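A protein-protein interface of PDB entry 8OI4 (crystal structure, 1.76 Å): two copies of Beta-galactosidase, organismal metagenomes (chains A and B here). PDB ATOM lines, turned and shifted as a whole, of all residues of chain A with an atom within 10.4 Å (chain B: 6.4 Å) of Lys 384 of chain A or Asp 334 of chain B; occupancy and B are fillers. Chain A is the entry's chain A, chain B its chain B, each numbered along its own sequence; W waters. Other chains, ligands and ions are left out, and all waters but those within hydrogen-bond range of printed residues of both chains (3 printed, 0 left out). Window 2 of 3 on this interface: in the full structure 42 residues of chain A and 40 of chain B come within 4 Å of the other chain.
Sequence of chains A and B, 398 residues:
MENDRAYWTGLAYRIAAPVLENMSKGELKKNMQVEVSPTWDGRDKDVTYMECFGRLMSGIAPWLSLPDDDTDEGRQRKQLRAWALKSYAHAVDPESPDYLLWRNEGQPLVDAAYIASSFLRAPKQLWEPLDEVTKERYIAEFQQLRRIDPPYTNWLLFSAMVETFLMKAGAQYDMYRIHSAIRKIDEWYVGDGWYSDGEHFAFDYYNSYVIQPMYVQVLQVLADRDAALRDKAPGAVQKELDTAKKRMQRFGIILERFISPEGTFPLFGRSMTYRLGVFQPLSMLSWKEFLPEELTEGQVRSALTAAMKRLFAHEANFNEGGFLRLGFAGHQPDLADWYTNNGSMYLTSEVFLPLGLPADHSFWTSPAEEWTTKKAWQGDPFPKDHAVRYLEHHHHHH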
ATOM      1  N   ARG A 250     -20.862   1.596  11.583  1.00  0.00           N
ATOM      2  CA  ARG A 250     -21.069   0.576  12.590  1.00  0.00           C
ATOM      3  C   ARG A 250     -22.454  -0.055  12.452  1.00  0.00           C
ATOM      4  O   ARG A 250     -22.599  -1.275  12.519  1.00  0.00           O
ATOM      5  CB  ARG A 250     -20.847   1.153  13.981  1.00  0.00           C
ATOM      6  CG  ARG A 250     -21.225   0.184  15.101  1.00  0.00           C
ATOM      7  CD  ARG A 250     -20.383  -1.084  15.033  1.00  0.00           C
ATOM      8  NE  ARG A 250     -20.683  -1.961  16.162  1.00  0.00           N
ATOM      9  CZ  ARG A 250     -20.649  -3.288  16.132  1.00  0.00           C
ATOM     10  NH1 ARG A 250     -20.192  -3.947  15.084  1.00  0.00           N
ATOM     11  NH2 ARG A 250     -21.075  -3.969  17.192  1.00  0.00           N
ATOM     12  N   ILE A 253     -22.377  -2.524   9.649  1.00  0.00           N
ATOM     13  CA  ILE A 253     -21.785  -3.789  10.067  1.00  0.00           C
ATOM     14  C   ILE A 253     -22.820  -4.646  10.791  1.00  0.00           C
ATOM     15  O   ILE A 253     -22.907  -5.858  10.574  1.00  0.00           O
ATOM     16  CB  ILE A 253     -20.542  -3.533  10.931  1.00  0.00           C
ATOM     17  CG1 ILE A 253     -19.374  -2.966  10.095  1.00  0.00           C
ATOM     18  CG2 ILE A 253     -20.107  -4.798  11.722  1.00  0.00           C
ATOM     19  CD1 ILE A 253     -18.277  -2.356  10.917  1.00  0.00           C
ATOM     20  N   GLU A 256     -25.421  -6.041   8.260  1.00  0.00           N
ATOM     21  CA  GLU A 256     -24.916  -7.150   7.474  1.00  0.00           C
ATOM     22  C   GLU A 256     -24.937  -8.439   8.296  1.00  0.00           C
ATOM     23  O   GLU A 256     -25.271  -9.498   7.767  1.00  0.00           O
ATOM     24  CB  GLU A 256     -23.525  -6.841   6.917  1.00  0.00           C
ATOM     25  CG  GLU A 256     -22.974  -7.911   5.968  1.00  0.00           C
ATOM     26  CD  GLU A 256     -22.189  -9.059   6.609  1.00  0.00           C
ATOM     27  OE1 GLU A 256     -21.935  -9.026   7.839  1.00  0.00           O
ATOM     28  OE2 GLU A 256     -21.814  -9.991   5.861  1.00  0.00           O
ATOM     29  N   ARG A 257     -24.640  -8.316   9.596  1.00  0.00           N
ATOM     30  CA  ARG A 257     -24.656  -9.457  10.502  1.00  0.00           C
ATOM     31  C   ARG A 257     -26.061  -9.926  10.887  1.00  0.00           C
ATOM     32  O   ARG A 257     -26.206 -10.981  11.493  1.00  0.00           O
ATOM     33  CB  ARG A 257     -23.845  -9.115  11.746  1.00  0.00           C
ATOM     34  CG  ARG A 257     -22.348  -9.253  11.479  1.00  0.00           C
ATOM     35  CD  ARG A 257     -21.528  -8.468  12.457  1.00  0.00           C
ATOM     36  NE  ARG A 257     -20.107  -8.764  12.314  1.00  0.00           N
ATOM     37  CZ  ARG A 257     -19.474  -9.792  12.857  1.00  0.00           C
ATOM     38  NH1 ARG A 257     -20.096 -10.676  13.626  1.00  0.00           N
ATOM     39  NH2 ARG A 257     -18.172  -9.920  12.648  1.00  0.00           N
ATOM     40  N   GLU A 293     -13.897  -0.958   6.399  1.00  0.00           N
ATOM     41  CA  GLU A 293     -13.006  -2.005   5.911  1.00  0.00           C
ATOM     42  C   GLU A 293     -13.471  -3.415   6.278  1.00  0.00           C
ATOM     43  O   GLU A 293     -13.133  -4.363   5.574  1.00  0.00           O
ATOM     44  CB  GLU A 293     -11.581  -1.801   6.429  1.00  0.00           C
ATOM     45  CG  GLU A 293     -11.465  -1.874   7.951  1.00  0.00           C
ATOM     46  CD  GLU A 293     -10.098  -1.458   8.498  1.00  0.00           C
ATOM     47  OE1 GLU A 293      -9.110  -1.425   7.722  1.00  0.00           O
ATOM     48  OE2 GLU A 293     -10.026  -1.135   9.709  1.00  0.00           O
ATOM     49  N   GLU A 294     -14.260  -3.545   7.358  1.00  0.00           N
ATOM     50  CA  GLU A 294     -14.855  -4.821   7.739  1.00  0.00           C
ATOM     51  C   GLU A 294     -15.793  -5.424   6.685  1.00  0.00           C
ATOM     52  O   GLU A 294     -16.047  -6.619   6.718  1.00  0.00           O
ATOM     53  CB  GLU A 294     -15.687  -4.677   9.049  1.00  0.00           C
ATOM     54  CG  GLU A 294     -14.865  -4.410  10.300  1.00  0.00           C
ATOM     55  CD  GLU A 294     -14.448  -2.976  10.583  1.00  0.00           C
ATOM     56  OE1 GLU A 294     -14.536  -2.110   9.686  1.00  0.00           O
ATOM     57  OE2 GLU A 294     -14.092  -2.712  11.756  1.00  0.00           O
ATOM     58  N   LEU A 295     -16.331  -4.590   5.777  1.00  0.00           N
ATOM     59  CA  LEU A 295     -17.304  -5.020   4.789  1.00  0.00           C
ATOM     60  C   LEU A 295     -16.766  -4.827   3.377  1.00  0.00           C
ATOM     61  O   LEU A 295     -16.355  -3.726   3.024  1.00  0.00           O
ATOM     62  CB  LEU A 295     -18.575  -4.201   4.922  1.00  0.00           C
ATOM     63  CG  LEU A 295     -19.402  -4.452   6.176  1.00  0.00           C
ATOM     64  CD1 LEU A 295     -20.601  -3.521   6.230  1.00  0.00           C
ATOM     65  CD2 LEU A 295     -19.811  -5.882   6.237  1.00  0.00           C
ATOM     66  N   GLN A 299     -19.488  -8.798  -0.518  1.00  0.00           N
ATOM     67  CA  GLN A 299     -20.252  -9.469   0.522  1.00  0.00           C
ATOM     68  C   GLN A 299     -21.566  -8.731   0.739  1.00  0.00           C
ATOM     69  O   GLN A 299     -22.597  -9.372   0.931  1.00  0.00           O
ATOM     70  CB  GLN A 299     -19.432  -9.680   1.822  1.00  0.00           C
ATOM     71  CG  GLN A 299     -19.743  -8.812   2.966  1.00  0.00           C
ATOM     72  CD  GLN A 299     -18.724  -8.962   4.080  1.00  0.00           C
ATOM     73  OE1 GLN A 299     -17.579  -8.492   3.952  1.00  0.00           O
ATOM     74  NE2 GLN A 299     -19.144  -9.559   5.210  1.00  0.00           N
ATOM     75  N   THR A 372     -21.300 -12.772   6.648  1.00  0.00           N
ATOM     76  CA  THR A 372     -20.793 -13.236   7.922  1.00  0.00           C
ATOM     77  C   THR A 372     -21.479 -14.496   8.432  1.00  0.00           C
ATOM     78  O   THR A 372     -20.798 -15.467   8.767  1.00  0.00           O
ATOM     79  CB  THR A 372     -20.890 -12.117   8.964  1.00  0.00           C
ATOM     80  OG1 THR A 372     -20.216 -10.968   8.450  1.00  0.00           O
ATOM     81  CG2 THR A 372     -20.295 -12.520  10.281  1.00  0.00           C
ATOM     82  N   LYS A 375     -20.743 -17.672   6.346  1.00  0.00           N
ATOM     83  CA  LYS A 375     -19.465 -18.265   6.710  1.00  0.00           C
ATOM     84  C   LYS A 375     -19.569 -19.001   8.047  1.00  0.00           C
ATOM     85  O   LYS A 375     -19.118 -20.135   8.180  1.00  0.00           O
ATOM     86  CB  LYS A 375     -18.382 -17.187   6.779  1.00  0.00           C
ATOM     87  CG  LYS A 375     -17.987 -16.652   5.399  1.00  0.00           C
ATOM     88  CD  LYS A 375     -16.903 -15.556   5.474  1.00  0.00           C
ATOM     89  CE  LYS A 375     -17.396 -14.317   6.157  1.00  0.00           C
ATOM     90  NZ  LYS A 375     -16.389 -13.226   6.085  1.00  0.00           N
ATOM     91  N   ALA A 376     -20.190 -18.337   9.035  1.00  0.00           N
ATOM     92  CA  ALA A 376     -20.246 -18.857  10.393  1.00  0.00           C
ATOM     93  C   ALA A 376     -20.920 -20.227  10.445  1.00  0.00           C
ATOM     94  O   ALA A 376     -20.343 -21.181  10.967  1.00  0.00           O
ATOM     95  CB  ALA A 376     -20.957 -17.871  11.284  1.00  0.00           C
ATOM     96  N   GLY A 379     -19.238 -23.397   9.319  1.00  0.00           N
ATOM     97  CA  GLY A 379     -18.113 -23.830  10.118  1.00  0.00           C
ATOM     98  C   GLY A 379     -16.775 -23.228   9.690  1.00  0.00           C
ATOM     99  O   GLY A 379     -15.730 -23.672  10.144  1.00  0.00           O
ATOM    100  N   ASP A 380     -16.829 -22.195   8.850  1.00  0.00           N
ATOM    101  CA  ASP A 380     -15.653 -21.545   8.305  1.00  0.00           C
ATOM    102  C   ASP A 380     -15.222 -20.367   9.175  1.00  0.00           C
ATOM    103  O   ASP A 380     -16.016 -19.866   9.971  1.00  0.00           O
ATOM    104  CB  ASP A 380     -15.954 -21.061   6.885  1.00  0.00           C
ATOM    105  CG  ASP A 380     -16.131 -22.230   5.890  1.00  0.00           C
ATOM    106  OD1 ASP A 380     -15.649 -23.348   6.193  1.00  0.00           O
ATOM    107  OD2 ASP A 380     -16.779 -22.034   4.841  1.00  0.00           O
ATOM    108  N   PRO A 381     -13.964 -19.888   9.052  1.00  0.00           N
ATOM    109  CA  PRO A 381     -13.544 -18.676   9.765  1.00  0.00           C
ATOM    110  C   PRO A 381     -14.439 -17.492   9.437  1.00  0.00           C
ATOM    111  O   PRO A 381     -14.867 -17.315   8.295  1.00  0.00           O
ATOM    112  CB  PRO A 381     -12.086 -18.456   9.300  1.00  0.00           C
ATOM    113  CG  PRO A 381     -11.617 -19.859   8.877  1.00  0.00           C
ATOM    114  CD  PRO A 381     -12.871 -20.520   8.283  1.00  0.00           C
ATOM    115  N   PHE A 382     -14.758 -16.706  10.466  1.00  0.00           N
ATOM    116  CA  PHE A 382     -15.448 -15.448  10.266  1.00  0.00           C
ATOM    117  C   PHE A 382     -14.959 -14.475  11.336  1.00  0.00           C
ATOM    118  O   PHE A 382     -14.519 -14.896  12.401  1.00  0.00           O
ATOM    119  CB  PHE A 382     -16.970 -15.615  10.269  1.00  0.00           C
ATOM    120  CG  PHE A 382     -17.603 -16.000  11.579  1.00  0.00           C
ATOM    121  CD1 PHE A 382     -17.539 -17.303  12.040  1.00  0.00           C
ATOM    122  CD2 PHE A 382     -18.265 -15.055  12.350  1.00  0.00           C
ATOM    123  CE1 PHE A 382     -18.154 -17.668  13.246  1.00  0.00           C
ATOM    124  CE2 PHE A 382     -18.882 -15.418  13.544  1.00  0.00           C
ATOM    125  CZ  PHE A 382     -18.820 -16.717  13.987  1.00  0.00           C
ATOM    126  N   PRO A 383     -15.005 -13.155  11.078  1.00  0.00           N
ATOM    127  CA  PRO A 383     -14.406 -12.186  11.997  1.00  0.00           C
ATOM    128  C   PRO A 383     -15.119 -11.999  13.332  1.00  0.00           C
ATOM    129  O   PRO A 383     -16.346 -12.061  13.414  1.00  0.00           O
ATOM    130  CB  PRO A 383     -14.426 -10.863  11.203  1.00  0.00           C
ATOM    131  CG  PRO A 383     -15.088 -11.157   9.891  1.00  0.00           C
ATOM    132  CD  PRO A 383     -15.636 -12.547   9.899  1.00  0.00           C
ATOM    133  N   LYS A 384     -14.302 -11.758  14.362  1.00  0.00           N
ATOM    134  CA  LYS A 384     -14.755 -11.230  15.634  1.00  0.00           C
ATOM    135  C   LYS A 384     -15.398  -9.870  15.403  1.00  0.00           C
ATOM    136  O   LYS A 384     -14.956  -9.115  14.534  1.00  0.00           O
ATOM    137  CB  LYS A 384     -13.589 -11.058  16.628  1.00  0.00           C
ATOM    138  CG  LYS A 384     -13.107 -12.333  17.221  1.00  0.00           C
ATOM    139  CD  LYS A 384     -12.203 -12.085  18.450  1.00  0.00           C
ATOM    140  CE  LYS A 384     -10.904 -11.433  18.110  1.00  0.00           C
ATOM    141  NZ  LYS A 384     -10.146 -12.257  17.161  1.00  0.00           N
ATOM    142  N   ASP A 385     -16.444  -9.580  16.180  1.00  0.00           N
ATOM    143  CA  ASP A 385     -17.069  -8.266  16.167  1.00  0.00           C
ATOM    144  C   ASP A 385     -16.656  -7.524  17.437  1.00  0.00           C
ATOM    145  O   ASP A 385     -16.359  -8.148  18.452  1.00  0.00           O
ATOM    146  CB  ASP A 385     -18.598  -8.390  16.081  1.00  0.00           C
ATOM    147  CG  ASP A 385     -19.320  -7.077  15.788  1.00  0.00           C
ATOM    148  OD1 ASP A 385     -18.841  -6.313  14.914  1.00  0.00           O
ATOM    149  OD2 ASP A 385     -20.391  -6.841  16.384  1.00  0.00           O
ATOM    150  N   HIS A 386     -16.625  -6.194  17.378  1.00  0.00           N
ATOM    151  CA  HIS A 386     -16.241  -5.362  18.509  1.00  0.00           C
ATOM    152  C   HIS A 386     -17.139  -4.125  18.518  1.00  0.00           C
ATOM    153  O   HIS A 386     -17.510  -3.620  17.467  1.00  0.00           O
ATOM    154  CB  HIS A 386     -14.757  -4.950  18.465  1.00  0.00           C
ATOM    155  CG  HIS A 386     -14.281  -4.361  17.179  1.00  0.00           C
ATOM    156  ND1 HIS A 386     -14.122  -3.003  16.979  1.00  0.00           N
ATOM    157  CD2 HIS A 386     -13.949  -4.948  16.019  1.00  0.00           C
ATOM    158  CE1 HIS A 386     -13.714  -2.782  15.735  1.00  0.00           C
ATOM    159  NE2 HIS A 386     -13.608  -3.950  15.128  1.00  0.00           N
ATOM    160  N   ALA A 387     -17.493  -3.675  19.718  1.00  0.00           N
ATOM    161  CA  ALA A 387     -18.217  -2.439  19.911  1.00  0.00           C
ATOM    162  C   ALA A 387     -17.357  -1.267  19.459  1.00  0.00           C
ATOM    163  O   ALA A 387     -16.140  -1.295  19.585  1.00  0.00           O
ATOM    164  CB  ALA A 387     -18.592  -2.274  21.381  1.00  0.00           C
ATOM    165  N   VAL A 388     -18.018  -0.215  18.988  1.00  0.00           N
ATOM    166  CA  VAL A 388     -17.380   1.084  18.857  1.00  0.00           C
ATOM    167  C   VAL A 388     -18.022   1.970  19.925  1.00  0.00           C
ATOM    168  O   VAL A 388     -19.198   2.328  19.817  1.00  0.00           O
ATOM    169  CB  VAL A 388     -17.523   1.633  17.405  1.00  0.00           C
ATOM    170  CG1 VAL A 388     -17.010   0.626  16.386  1.00  0.00           C
ATOM    171  CG2 VAL A 388     -18.940   2.013  17.093  1.00  0.00           C
ATOM    172  N   SER B  37      -7.352 -19.115  23.337  1.00  0.00           N
ATOM    173  CA  SER B  37      -7.443 -18.195  22.220  1.00  0.00           C
ATOM    174  C   SER B  37      -6.111 -18.021  21.514  1.00  0.00           C
ATOM    175  O   SER B  37      -5.072 -17.940  22.167  1.00  0.00           O
ATOM    176  CB  SER B  37      -7.897 -16.819  22.700  1.00  0.00           C
ATOM    177  OG  SER B  37      -7.916 -15.905  21.613  1.00  0.00           O
ATOM    178  N   PRO B  38      -6.087 -17.915  20.166  1.00  0.00           N
ATOM    179  CA  PRO B  38      -4.858 -17.495  19.479  1.00  0.00           C
ATOM    180  C   PRO B  38      -4.309 -16.137  19.931  1.00  0.00           C
ATOM    181  O   PRO B  38      -3.131 -15.869  19.742  1.00  0.00           O
ATOM    182  CB  PRO B  38      -5.271 -17.486  17.995  1.00  0.00           C
ATOM    183  CG  PRO B  38      -6.493 -18.440  17.931  1.00  0.00           C
ATOM    184  CD  PRO B  38      -7.201 -18.219  19.246  1.00  0.00           C
ATOM    185  N   THR B  39      -5.155 -15.272  20.515  1.00  0.00           N
ATOM    186  CA  THR B  39      -4.701 -13.995  21.060  1.00  0.00           C
ATOM    187  C   THR B  39      -4.708 -13.960  22.591  1.00  0.00           C
ATOM    188  O   THR B  39      -4.935 -12.906  23.184  1.00  0.00           O
ATOM    189  CB  THR B  39      -5.545 -12.856  20.491  1.00  0.00           C
ATOM    190  OG1 THR B  39      -6.936 -13.066  20.804  1.00  0.00           O
ATOM    191  CG2 THR B  39      -5.370 -12.720  18.943  1.00  0.00           C
ATOM    192  N   GLY B 269     -21.249  -8.475  18.281  1.00  0.00           N
ATOM    193  CA  GLY B 269     -20.654  -8.236  19.574  1.00  0.00           C
ATOM    194  C   GLY B 269     -19.589  -9.266  19.933  1.00  0.00           C
ATOM    195  O   GLY B 269     -19.384 -10.259  19.244  1.00  0.00           O
ATOM    196  N   LEU B 326     -13.044 -24.144  20.852  1.00  0.00           N
ATOM    197  CA  LEU B 326     -13.221 -22.731  20.527  1.00  0.00           C
ATOM    198  C   LEU B 326     -13.892 -22.583  19.167  1.00  0.00           C
ATOM    199  O   LEU B 326     -13.364 -23.037  18.155  1.00  0.00           O
ATOM    200  CB  LEU B 326     -11.877 -22.025  20.490  1.00  0.00           C
ATOM    201  CG  LEU B 326     -11.133 -21.939  21.815  1.00  0.00           C
ATOM    202  CD1 LEU B 326      -9.821 -21.231  21.631  1.00  0.00           C
ATOM    203  CD2 LEU B 326     -11.959 -21.249  22.895  1.00  0.00           C
ATOM    204  N   GLN B 332     -13.646 -22.717  15.221  1.00  0.00           N
ATOM    205  CA  GLN B 332     -13.377 -21.413  14.630  1.00  0.00           C
ATOM    206  C   GLN B 332     -12.575 -20.647  15.674  1.00  0.00           C
ATOM    207  O   GLN B 332     -13.102 -19.750  16.330  1.00  0.00           O
ATOM    208  CB  GLN B 332     -14.701 -20.708  14.266  1.00  0.00           C
ATOM    209  CG  GLN B 332     -15.461 -21.426  13.145  1.00  0.00           C
ATOM    210  CD  GLN B 332     -16.959 -21.213  13.167  1.00  0.00           C
ATOM    211  OE1 GLN B 332     -17.589 -21.307  14.215  1.00  0.00           O
ATOM    212  NE2 GLN B 332     -17.583 -20.968  12.025  1.00  0.00           N
ATOM    213  N   PRO B 333     -11.299 -21.038  15.898  1.00  0.00           N
ATOM    214  CA  PRO B 333     -10.553 -20.563  17.064  1.00  0.00           C
ATOM    215  C   PRO B 333     -10.257 -19.064  17.045  1.00  0.00           C
ATOM    216  O   PRO B 333     -10.141 -18.449  18.103  1.00  0.00           O
ATOM    217  CB  PRO B 333      -9.274 -21.416  17.038  1.00  0.00           C
ATOM    218  CG  PRO B 333      -9.100 -21.796  15.568  1.00  0.00           C
ATOM    219  CD  PRO B 333     -10.514 -21.949  15.044  1.00  0.00           C
ATOM    220  N   ASP B 334     -10.153 -18.474  15.853  1.00  0.00           N
ATOM    221  CA  ASP B 334      -9.867 -17.049  15.752  1.00  0.00           C
ATOM    222  C   ASP B 334     -11.040 -16.166  16.175  1.00  0.00           C
ATOM    223  O   ASP B 334     -10.856 -14.971  16.387  1.00  0.00           O
ATOM    224  CB  ASP B 334      -9.387 -16.684  14.341  1.00  0.00           C
ATOM    225  CG  ASP B 334      -8.005 -17.259  14.065  1.00  0.00           C
ATOM    226  OD1 ASP B 334      -7.070 -16.966  14.842  1.00  0.00           O
ATOM    227  OD2 ASP B 334      -7.861 -17.993  13.092  1.00  0.00           O
ATOM    228  N   LEU B 335     -12.220 -16.763  16.366  1.00  0.00           N
ATOM    229  CA  LEU B 335     -13.360 -16.073  16.947  1.00  0.00           C
ATOM    230  C   LEU B 335     -13.199 -15.801  18.445  1.00  0.00           C
ATOM    231  O   LEU B 335     -13.902 -14.975  19.017  1.00  0.00           O
ATOM    232  CB  LEU B 335     -14.599 -16.931  16.682  1.00  0.00           C
ATOM    233  CG  LEU B 335     -15.909 -16.272  16.913  1.00  0.00           C
ATOM    234  CD1 LEU B 335     -16.137 -15.154  15.888  1.00  0.00           C
ATOM    235  CD2 LEU B 335     -17.036 -17.295  16.852  1.00  0.00           C
ATOM    236  N   ALA B 336     -12.271 -16.518  19.083  1.00  0.00           N
ATOM    237  CA  ALA B 336     -12.047 -16.393  20.509  1.00  0.00           C
ATOM    238  C   ALA B 336     -11.326 -15.089  20.843  1.00  0.00           C
ATOM    239  O   ALA B 336     -10.310 -14.770  20.244  1.00  0.00           O
ATOM    240  CB  ALA B 336     -11.247 -17.579  21.021  1.00  0.00           C
ATOM    241  N   ASP B 337     -11.879 -14.350  21.810  1.00  0.00           N
ATOM    242  CA  ASP B 337     -11.295 -13.112  22.296  1.00  0.00           C
ATOM    243  C   ASP B 337     -10.060 -13.437  23.130  1.00  0.00           C
ATOM    244  O   ASP B 337      -9.791 -14.598  23.443  1.00  0.00           O
ATOM    245  CB  ASP B 337     -12.383 -12.316  23.087  1.00  0.00           C
ATOM    246  CG  ASP B 337     -13.558 -11.834  22.235  1.00  0.00           C
ATOM    247  OD1 ASP B 337     -13.378 -10.866  21.454  1.00  0.00           O
ATOM    248  OD2 ASP B 337     -14.647 -12.443  22.318  1.00  0.00           O
ATOM    249  N   TRP B 338      -9.283 -12.412  23.477  1.00  0.00           N
ATOM    250  CA  TRP B 338      -8.035 -12.604  24.209  1.00  0.00           C
ATOM    251  C   TRP B 338      -8.218 -13.217  25.602  1.00  0.00           C
ATOM    252  O   TRP B 338      -7.281 -13.777  26.157  1.00  0.00           O
ATOM    253  CB  TRP B 338      -7.223 -11.262  24.314  1.00  0.00           C
ATOM    254  CG  TRP B 338      -8.022 -10.069  24.750  1.00  0.00           C
ATOM    255  CD1 TRP B 338      -8.774  -9.247  23.958  1.00  0.00           C
ATOM    256  CD2 TRP B 338      -8.185  -9.595  26.086  1.00  0.00           C
ATOM    257  NE1 TRP B 338      -9.391  -8.288  24.722  1.00  0.00           N
ATOM    258  CE2 TRP B 338      -9.045  -8.477  26.035  1.00  0.00           C
ATOM    259  CE3 TRP B 338      -7.690 -10.005  27.329  1.00  0.00           C
ATOM    260  CZ2 TRP B 338      -9.410  -7.763  27.176  1.00  0.00           C
ATOM    261  CZ3 TRP B 338      -8.059  -9.293  28.461  1.00  0.00           C
ATOM    262  CH2 TRP B 338      -8.903  -8.189  28.378  1.00  0.00           C
HETATM  263  O   HOH W   1     -17.584 -11.660  17.835  1.00  0.00           O
HETATM  264  O   HOH W   2      -8.219 -14.621  18.607  1.00  0.00           O
HETATM  265  O   HOH W   3     -14.456  -8.777  19.950  1.00  0.00           O
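OD2 of Asp 385 of chain A is in hydrogen-bond range of N of Gly 269 of chain B (2.6 Å).
NZ of Lys 384 of chain A sits at hydrogen-bond distance from O of Asp 334 of chain B, 2.9 Å away.
NE2 of Gln 332 of chain B lies within hydrogen-bond range of O of Asp 380 of chain A (2.8 Å).
NE2 of Gln 332 of chain B lies within hydrogen-bond range of O of Ala 376 of chain A, at 3.0 Å.
OD1 of Asp 385 of chain A lies within salt-bridge range of NH1 of Arg 250 of chain A (2.7 Å).
The side-chain hydroxyl (OG) of Ser 37 of chain B lies within hydrogen-bond range of the backbone carbonyl oxygen (O) of Ala 336 of chain B.
O of Lys 375 of chain A is in hydrogen-bond range of N of Asp 380 of chain A, at 3.2 Å.
OG of Ser 37 of chain B is in hydrogen-bond range of O of Asp 337 of chain B.
The guanidinium group (NH2) of Arg 257 of chain A is in hydrogen-bond range of the backbone carbonyl oxygen (O) of Pro 383 of chain A, at 2.9 Å.
The side-chain carboxylate (OD1) of Asp 385 of chain A is in salt-bridge range of the guanidinium group (NE) of Arg 257 of chain A, 3.8 Å away.
NE2 of Gln 332 of chain B touches C of Gly 379 of chain A, 3.3 Å away.
Phe 382 of chain A touches Gln 332 of chain B.
Phe 382 of chain A touches Leu 335 of chain B.
O of Pro 383 of chain A touches CD1 of Leu 335 of chain B, 3.97 Å away.
O of Leu 335 of chain B touches CG of Lys 384 of chain A, 3.3 Å away.
Lys 384 of chain A touches Ala 336 of chain B (CD to O, 3.7 Å).
Lys 384 of chain A touches Asp 337 of chain B (CD to OD1, 3.4 Å).
Lys 384 of chain A touches just these residues of chain B: Asp 334, Leu 335, Ala 336 and Asp 337.
Printed residues of chain A within 4 Å of Asp 334 of chain B: Lys 384 (2.9 Å).
No residue of chain A comes within 4 Å of Pro 333 of chain B.
Leu 335 of chain B touches just these residues of chain A: Phe 382, Pro 383 and Lys 384.
Ala 336 of chain B touches one residue of chain A.
Of chain A, only Lys 384 comes within 4 Å of Asp 337 of chain B.
Printed residues of chain B within 4 Å of Ala 376 of chain A: Gln 332 (3.0 Å).
Of the printed residues of chain A, Gln 332 of chain B touches Ala 376, Gly 379, Asp 380 and Phe 382.
Of the printed residues of chain B, Asp 380 of chain A touches Gln 332.
Of the printed residues of chain A, Gly 269 of chain B touches Asp 385.
Printed residues of chain B within 4 Å of Asp 385 of chain A: Gly 269.
The nearest residue of chain A that does not touch Asp 334 of chain B is Phe 382 of chain A (5.3 Å).
The nearest printed residue of chain B that does not touch Asp 385 of chain A is Asp 337 of chain B (5.0 Å).
Hydrophobic or aromatic side chains of chain B within 4 Å of the printed part of chain A: Leu 335.
Among the printed residues, no Asp or Glu carboxylate lies within 4 Å of a Lys or Arg side-chain nitrogen of the other chain.
No position is printed for both chains.
Water W3 lies within hydrogen-bond range of the backbone carbonyl oxygen of Asp 385 of chain A (2.5 Å) and the side-chain carboxylate of Asp 337 of chain B (2.8 Å).
Water W2 lies within hydrogen-bond range of the backbone carbonyl oxygen of Ala 336 of chain B (2.7 Å), the side-chain hydroxyl of Thr 39 of chain B (3.0 Å), the side-chain hydroxyl of Ser 37 of chain B (3.3 Å), the side-chain amino group of Lys 384 of chain A (3.4 Å) and the backbone carbonyl oxygen of Asp 334 of chain B (3.5 Å).
Water W1 bridges the backbone carbonyl oxygen (O) of Gly 269 of chain B (2.7 Å) and the backbone NH (N) of Asp 385 of chain A (2.9 Å).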
